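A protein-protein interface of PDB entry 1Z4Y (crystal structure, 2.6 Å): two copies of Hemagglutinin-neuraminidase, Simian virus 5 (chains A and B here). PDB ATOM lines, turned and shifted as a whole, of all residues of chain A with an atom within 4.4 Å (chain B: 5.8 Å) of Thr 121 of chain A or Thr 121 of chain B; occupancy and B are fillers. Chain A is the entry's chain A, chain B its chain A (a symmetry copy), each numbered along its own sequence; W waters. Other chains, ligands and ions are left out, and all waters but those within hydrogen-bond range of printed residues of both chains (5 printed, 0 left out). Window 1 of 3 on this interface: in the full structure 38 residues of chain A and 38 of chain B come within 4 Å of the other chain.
Water W5 bridges OE1 of Gln 521 of chain A (2.8 Å) and N of Leu 517 of chain B (3.1 Å).
Water W2 lies within hydrogen-bond range of the backbone carbonyl oxygen (O) of Ile 119 of chain A (2.8 Å), the backbone NH (N) of Thr 121 of chain B (2.9 Å) and the side-chain hydroxyl (OG) of Ser 117 of chain A (3.4 Å).
Water W3 lies within hydrogen-bond range of the backbone carbonyl oxygen (O) of Ile 119 of chain B (2.8 Å), the backbone NH (N) of Thr 121 of chain A (2.9 Å) and the side-chain hydroxyl (OG) of Ser 117 of chain B (3.4 Å).
Water W1 lies within hydrogen-bond range of the backbone carbonyl oxygen (O) of Met 115 of chain B (3.0 Å), the side-chain amide nitrogen (ND2) of Asn 114 of chain B (3.4 Å) and the backbone carbonyl oxygen (O) of Thr 121 of chain A (3.5 Å).
Water W4 bridges O of Met 115 of chain A (3.0 Å) and O of Thr 121 of chain B (3.5 Å).
Met 115 of chain A touches Thr 121 of chain B, and with the chains exchanged Thr 121 of chain A touches Met 115 of chain B.
Met 115 of chain A touches Thr 123 of chain B, and with the chains exchanged Thr 123 of chain A touches Met 115 of chain B.
Ser 117 of chain A touches Pro 120 of chain B, and with the chains exchanged Pro 120 of chain A touches Ser 117 of chain B.
Thr 121 of chain A touches Gln 521 of chain B, and with the chains exchanged Gln 521 of chain A touches Thr 121 of chain B.
Of the 15 pairs that touch across the chains among the printed residues, 13 have their exchanged pair printed and touching as well.
The side-chain hydroxyl of Thr 123 of chain B lies within hydrogen-bond range of the backbone NH of Met 115 of chain A.
N of Ser 117 of chain A is in hydrogen-bond range of O of Thr 121 of chain B (2.8 Å).
O of Thr 121 of chain A sits at hydrogen-bond distance from N of Ser 117 of chain B.
The backbone NH (N) of Thr 123 of chain A is in hydrogen-bond range of the side-chain amide oxygen (OD1) of Asn 114 of chain B.
The side-chain hydroxyl (OG1) of Thr 123 of chain A sits at hydrogen-bond distance from the backbone NH (N) of Met 115 of chain B.
The backbone NH of Ile 119 of chain A sits at hydrogen-bond distance from the side-chain hydroxyl of Ser 117 of chain A (3.2 Å).
OG of Ser 117 of chain B lies within hydrogen-bond range of N of Ile 119 of chain B, at 3.2 Å.
Met 115 of chain A touches Thr 121 of chain B.
Pro 116 of chain A touches Thr 121 of chain B (C to O, 3.7 Å).
Ser 117 of chain A touches Pro 120 of chain B (O to CB, 3.4 Å).
Pro 120 of chain A touches Ser 117 of chain B (CB to O, 3.4 Å).
Met 115 of chain B touches Thr 121 of chain A.
Thr 121 of chain A touches Pro 116 of chain B.
OG1 of Thr 121 of chain A touches OG1 of Thr 121 of chain B (3.9 Å).
NE2 of Gln 521 of chain B touches CG2 of Thr 121 of chain A, at 3.3 Å.
Ala 122 of chain A touches Asn 114 of chain B (CB to OD1, 3.2 Å).
NE2 of Gln 521 of chain A touches CG2 of Thr 121 of chain B, 3.3 Å away.
Of the printed residues of chain A, Gln 521 of chain B touches Thr 121.
Printed residues of chain B within 4 Å of Met 115 of chain A: Thr 121 (3.6 Å) and Thr 123 (2.9 Å).
Of the printed residues of chain B, Gln 521 of chain A touches Thr 121 (3.3 Å).
Val 523 of chain B touches none of the printed residues of chain A.
Ile 119 of chain B touches none of the printed residues of chain A.
The nearest residue of chain B that does not touch Thr 121 of chain A is Asn 114 of chain B (5.4 Å).
Of the 14 printed residues of chain B, 8 touch a printed residue of chain A.
Hydrophobic or aromatic side chains of chain B within 4 Å of the printed part of chain A: Met 115 and Pro 120.
Hydrophobic or aromatic side chains of chain A within 4 Å of the printed part of chain B: Met 115, Pro 120 and Ala 122.
Among the printed residues, 15 pairs touch across the chains.
Among the printed residues, no Asp or Glu carboxylate lies within 4 Å of a Lys or Arg side-chain nitrogen of the other chain.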
ATOM      1  N   MET A 115      18.446  -0.601  34.524  1.00  0.00           N
ATOM      2  CA  MET A 115      17.176  -1.303  34.646  1.00  0.00           C
ATOM      3  C   MET A 115      16.206  -0.705  33.624  1.00  0.00           C
ATOM      4  O   MET A 115      16.443   0.379  33.104  1.00  0.00           O
ATOM      5  CB  MET A 115      16.601  -1.129  36.060  1.00  0.00           C
ATOM      6  CG  MET A 115      15.971   0.233  36.320  1.00  0.00           C
ATOM      7  SD  MET A 115      15.374   0.449  38.011  1.00  0.00           S
ATOM      8  CE  MET A 115      15.121   2.215  38.063  1.00  0.00           C
ATOM      9  N   PRO A 116      15.118  -1.422  33.297  1.00  0.00           N
ATOM     10  CA  PRO A 116      14.172  -0.853  32.332  1.00  0.00           C
ATOM     11  C   PRO A 116      13.471   0.317  33.022  1.00  0.00           C
ATOM     12  O   PRO A 116      12.975   0.170  34.137  1.00  0.00           O
ATOM     13  CB  PRO A 116      13.211  -2.008  32.061  1.00  0.00           C
ATOM     14  CG  PRO A 116      14.064  -3.218  32.284  1.00  0.00           C
ATOM     15  CD  PRO A 116      14.831  -2.849  33.530  1.00  0.00           C
ATOM     16  N   SER A 117      13.439   1.472  32.367  1.00  0.00           N
ATOM     17  CA  SER A 117      12.813   2.647  32.947  1.00  0.00           C
ATOM     18  C   SER A 117      11.300   2.527  32.975  1.00  0.00           C
ATOM     19  O   SER A 117      10.688   2.118  31.989  1.00  0.00           O
ATOM     20  CB  SER A 117      13.209   3.902  32.163  1.00  0.00           C
ATOM     21  OG  SER A 117      12.562   5.050  32.685  1.00  0.00           O
ATOM     22  N   ILE A 119       9.447   5.154  33.550  1.00  0.00           N
ATOM     23  CA  ILE A 119       8.978   6.509  33.258  1.00  0.00           C
ATOM     24  C   ILE A 119       8.953   6.699  31.747  1.00  0.00           C
ATOM     25  O   ILE A 119       9.994   6.707  31.093  1.00  0.00           O
ATOM     26  CB  ILE A 119       9.893   7.558  33.908  1.00  0.00           C
ATOM     27  CG1 ILE A 119       9.971   7.300  35.415  1.00  0.00           C
ATOM     28  CG2 ILE A 119       9.360   8.948  33.640  1.00  0.00           C
ATOM     29  CD1 ILE A 119      10.886   8.225  36.158  1.00  0.00           C
ATOM     30  N   PRO A 120       7.754   6.854  31.176  1.00  0.00           N
ATOM     31  CA  PRO A 120       7.539   7.037  29.740  1.00  0.00           C
ATOM     32  C   PRO A 120       8.190   8.253  29.089  1.00  0.00           C
ATOM     33  O   PRO A 120       8.235   9.347  29.646  1.00  0.00           O
ATOM     34  CB  PRO A 120       6.020   7.042  29.620  1.00  0.00           C
ATOM     35  CG  PRO A 120       5.592   7.645  30.911  1.00  0.00           C
ATOM     36  CD  PRO A 120       6.479   6.949  31.906  1.00  0.00           C
ATOM     37  N   THR A 121       8.674   8.023  27.879  1.00  0.00           N
ATOM     38  CA  THR A 121       9.359   9.013  27.065  1.00  0.00           C
ATOM     39  C   THR A 121       8.428   9.686  26.049  1.00  0.00           C
ATOM     40  O   THR A 121       7.384   9.144  25.700  1.00  0.00           O
ATOM     41  CB  THR A 121      10.533   8.306  26.340  1.00  0.00           C
ATOM     42  OG1 THR A 121      11.703   8.398  27.155  1.00  0.00           O
ATOM     43  CG2 THR A 121      10.799   8.890  24.978  1.00  0.00           C
ATOM     44  N   ALA A 122       8.808  10.872  25.587  1.00  0.00           N
ATOM     45  CA  ALA A 122       8.020  11.588  24.592  1.00  0.00           C
ATOM     46  C   ALA A 122       8.338  10.942  23.246  1.00  0.00           C
ATOM     47  O   ALA A 122       9.371  10.289  23.104  1.00  0.00           O
ATOM     48  CB  ALA A 122       8.407  13.060  24.577  1.00  0.00           C
ATOM     49  N   THR A 123       7.458  11.105  22.260  1.00  0.00           N
ATOM     50  CA  THR A 123       7.710  10.512  20.952  1.00  0.00           C
ATOM     51  C   THR A 123       7.894  11.548  19.852  1.00  0.00           C
ATOM     52  O   THR A 123       7.850  11.226  18.665  1.00  0.00           O
ATOM     53  CB  THR A 123       6.588   9.518  20.554  1.00  0.00           C
ATOM     54  OG1 THR A 123       5.305  10.155  20.636  1.00  0.00           O
ATOM     55  CG2 THR A 123       6.613   8.315  21.476  1.00  0.00           C
ATOM     56  N   GLN A 521      13.785  14.393  29.345  1.00  0.00           N
ATOM     57  CA  GLN A 521      13.624  12.957  29.473  1.00  0.00           C
ATOM     58  C   GLN A 521      13.751  12.775  30.970  1.00  0.00           C
ATOM     59  O   GLN A 521      14.801  13.055  31.538  1.00  0.00           O
ATOM     60  CB  GLN A 521      14.736  12.174  28.773  1.00  0.00           C
ATOM     61  CG  GLN A 521      14.486  10.655  28.800  1.00  0.00           C
ATOM     62  CD  GLN A 521      15.568   9.825  28.109  1.00  0.00           C
ATOM     63  OE1 GLN A 521      16.175  10.264  27.137  1.00  0.00           O
ATOM     64  NE2 GLN A 521      15.790   8.611  28.600  1.00  0.00           N
ATOM     65  N   ASN B 114       2.792  13.289  19.599  1.00  0.00           N
ATOM     66  CA  ASN B 114       3.427  12.958  20.870  1.00  0.00           C
ATOM     67  C   ASN B 114       2.560  12.218  21.877  1.00  0.00           C
ATOM     68  O   ASN B 114       1.625  12.784  22.431  1.00  0.00           O
ATOM     69  CB  ASN B 114       3.955  14.219  21.545  1.00  0.00           C
ATOM     70  CG  ASN B 114       4.738  13.911  22.799  1.00  0.00           C
ATOM     71  OD1 ASN B 114       5.871  13.433  22.735  1.00  0.00           O
ATOM     72  ND2 ASN B 114       4.132  14.153  23.948  1.00  0.00           N
ATOM     73  N   MET B 115       2.897  10.960  22.132  1.00  0.00           N
ATOM     74  CA  MET B 115       2.173  10.145  23.097  1.00  0.00           C
ATOM     75  C   MET B 115       3.188   9.581  24.094  1.00  0.00           C
ATOM     76  O   MET B 115       4.385   9.588  23.833  1.00  0.00           O
ATOM     77  CB  MET B 115       1.454   8.986  22.388  1.00  0.00           C
ATOM     78  CG  MET B 115       2.366   7.839  21.975  1.00  0.00           C
ATOM     79  SD  MET B 115       1.518   6.524  21.071  1.00  0.00           S
ATOM     80  CE  MET B 115       2.904   5.620  20.402  1.00  0.00           C
ATOM     81  N   PRO B 116       2.724   9.118  25.267  1.00  0.00           N
ATOM     82  CA  PRO B 116       3.683   8.559  26.225  1.00  0.00           C
ATOM     83  C   PRO B 116       4.184   7.237  25.644  1.00  0.00           C
ATOM     84  O   PRO B 116       3.385   6.398  25.235  1.00  0.00           O
ATOM     85  CB  PRO B 116       2.840   8.342  27.479  1.00  0.00           C
ATOM     86  CG  PRO B 116       1.786   9.398  27.366  1.00  0.00           C
ATOM     87  CD  PRO B 116       1.412   9.328  25.906  1.00  0.00           C
ATOM     88  N   SER B 117       5.500   7.058  25.599  1.00  0.00           N
ATOM     89  CA  SER B 117       6.075   5.843  25.047  1.00  0.00           C
ATOM     90  C   SER B 117       5.862   4.651  25.961  1.00  0.00           C
ATOM     91  O   SER B 117       6.062   4.747  27.171  1.00  0.00           O
ATOM     92  CB  SER B 117       7.574   6.031  24.798  1.00  0.00           C
ATOM     93  OG  SER B 117       8.159   4.836  24.310  1.00  0.00           O
ATOM     94  N   ILE B 119       7.535   1.888  25.483  1.00  0.00           N
ATOM     95  CA  ILE B 119       8.772   1.117  25.356  1.00  0.00           C
ATOM     96  C   ILE B 119       9.803   1.692  26.318  1.00  0.00           C
ATOM     97  O   ILE B 119      10.259   2.822  26.157  1.00  0.00           O
ATOM     98  CB  ILE B 119       9.306   1.170  23.917  1.00  0.00           C
ATOM     99  CG1 ILE B 119       8.226   0.665  22.956  1.00  0.00           C
ATOM    100  CG2 ILE B 119      10.554   0.324  23.795  1.00  0.00           C
ATOM    101  CD1 ILE B 119       8.605   0.725  21.507  1.00  0.00           C
ATOM    102  N   PRO B 120      10.181   0.913  27.337  1.00  0.00           N
ATOM    103  CA  PRO B 120      11.150   1.303  28.362  1.00  0.00           C
ATOM    104  C   PRO B 120      12.558   1.653  27.891  1.00  0.00           C
ATOM    105  O   PRO B 120      13.125   1.024  27.001  1.00  0.00           O
ATOM    106  CB  PRO B 120      11.123   0.122  29.325  1.00  0.00           C
ATOM    107  CG  PRO B 120      10.834  -1.027  28.425  1.00  0.00           C
ATOM    108  CD  PRO B 120       9.749  -0.481  27.538  1.00  0.00           C
ATOM    109  N   THR B 121      13.106   2.669  28.539  1.00  0.00           N
ATOM    110  CA  THR B 121      14.428   3.204  28.259  1.00  0.00           C
ATOM    111  C   THR B 121      15.502   2.641  29.197  1.00  0.00           C
ATOM    112  O   THR B 121      15.197   2.156  30.282  1.00  0.00           O
ATOM    113  CB  THR B 121      14.353   4.749  28.384  1.00  0.00           C
ATOM    114  OG1 THR B 121      14.031   5.302  27.106  1.00  0.00           O
ATOM    115  CG2 THR B 121      15.637   5.342  28.901  1.00  0.00           C
ATOM    116  N   ALA B 122      16.758   2.699  28.767  1.00  0.00           N
ATOM    117  CA  ALA B 122      17.865   2.226  29.588  1.00  0.00           C
ATOM    118  C   ALA B 122      18.145   3.326  30.608  1.00  0.00           C
ATOM    119  O   ALA B 122      17.766   4.476  30.393  1.00  0.00           O
ATOM    120  CB  ALA B 122      19.094   1.982  28.723  1.00  0.00           C
ATOM    121  N   THR B 123      18.791   2.986  31.721  1.00  0.00           N
ATOM    122  CA  THR B 123      19.087   3.995  32.731  1.00  0.00           C
ATOM    123  C   THR B 123      20.579   4.234  32.917  1.00  0.00           C
ATOM    124  O   THR B 123      21.005   4.847  33.896  1.00  0.00           O
ATOM    125  CB  THR B 123      18.438   3.643  34.094  1.00  0.00           C
ATOM    126  OG1 THR B 123      18.822   2.321  34.502  1.00  0.00           O
ATOM    127  CG2 THR B 123      16.929   3.716  33.982  1.00  0.00           C
ATOM    128  N   THR B 129      19.265  -1.737  24.716  1.00  0.00           N
ATOM    129  CA  THR B 129      17.921  -2.277  24.502  1.00  0.00           C
ATOM    130  C   THR B 129      17.791  -2.449  22.989  1.00  0.00           C
ATOM    131  O   THR B 129      17.871  -1.479  22.242  1.00  0.00           O
ATOM    132  CB  THR B 129      16.805  -1.325  25.000  1.00  0.00           C
ATOM    133  OG1 THR B 129      16.755  -0.147  24.188  1.00  0.00           O
ATOM    134  CG2 THR B 129      17.060  -0.925  26.436  1.00  0.00           C
ATOM    135  N   HIS B 145      11.407  -6.754  24.027  1.00  0.00           N
ATOM    136  CA  HIS B 145      12.724  -6.447  23.496  1.00  0.00           C
ATOM    137  C   HIS B 145      13.804  -6.998  24.414  1.00  0.00           C
ATOM    138  O   HIS B 145      13.554  -7.321  25.576  1.00  0.00           O
ATOM    139  CB  HIS B 145      12.903  -4.935  23.219  1.00  0.00           C
ATOM    140  CG  HIS B 145      13.076  -4.078  24.440  1.00  0.00           C
ATOM    141  ND1 HIS B 145      12.703  -2.749  24.457  1.00  0.00           N
ATOM    142  CD2 HIS B 145      13.617  -4.335  25.651  1.00  0.00           C
ATOM    143  CE1 HIS B 145      13.009  -2.229  25.633  1.00  0.00           C
ATOM    144  NE2 HIS B 145      13.564  -3.166  26.376  1.00  0.00           N
ATOM    145  N   LEU B 517      21.141   8.491  27.084  1.00  0.00           N
ATOM    146  CA  LEU B 517      20.929   7.243  27.821  1.00  0.00           C
ATOM    147  C   LEU B 517      20.870   6.009  26.918  1.00  0.00           C
ATOM    148  O   LEU B 517      20.101   5.969  25.964  1.00  0.00           O
ATOM    149  CB  LEU B 517      19.638   7.314  28.644  1.00  0.00           C
ATOM    150  CG  LEU B 517      19.619   8.001  30.013  1.00  0.00           C
ATOM    151  CD1 LEU B 517      20.497   7.238  30.984  1.00  0.00           C
ATOM    152  CD2 LEU B 517      20.084   9.435  29.886  1.00  0.00           C
ATOM    153  N   GLN B 521      17.759   3.726  21.750  1.00  0.00           N
ATOM    154  CA  GLN B 521      16.509   4.088  22.391  1.00  0.00           C
ATOM    155  C   GLN B 521      15.500   3.599  21.375  1.00  0.00           C
ATOM    156  O   GLN B 521      15.467   4.092  20.253  1.00  0.00           O
ATOM    157  CB  GLN B 521      16.355   5.600  22.568  1.00  0.00           C
ATOM    158  CG  GLN B 521      15.091   5.967  23.367  1.00  0.00           C
ATOM    159  CD  GLN B 521      14.891   7.468  23.577  1.00  0.00           C
ATOM    160  OE1 GLN B 521      15.852   8.222  23.694  1.00  0.00           O
ATOM    161  NE2 GLN B 521      13.636   7.896  23.650  1.00  0.00           N
ATOM    162  N   VAL B 523      12.162   3.744  19.928  1.00  0.00           N
ATOM    163  CA  VAL B 523      11.069   4.702  19.981  1.00  0.00           C
ATOM    164  C   VAL B 523       9.835   4.305  19.177  1.00  0.00           C
ATOM    165  O   VAL B 523       9.939   3.855  18.039  1.00  0.00           O
ATOM    166  CB  VAL B 523      11.544   6.079  19.471  1.00  0.00           C
ATOM    167  CG1 VAL B 523      10.399   7.067  19.485  1.00  0.00           C
ATOM    168  CG2 VAL B 523      12.702   6.575  20.322  1.00  0.00           C
HETATM  169  O   HOH W   1       4.898  11.551  25.989  1.00  0.00           O
HETATM  170  O   HOH W   2      11.257   4.736  29.513  1.00  0.00           O
HETATM  171  O   HOH W   3       9.662   5.300  27.374  1.00  0.00           O
HETATM  172  O   HOH W   4      16.817  -0.910  30.464  1.00  0.00           O
HETATM  173  O   HOH W   5      18.403   9.235  25.876  1.00  0.00           O
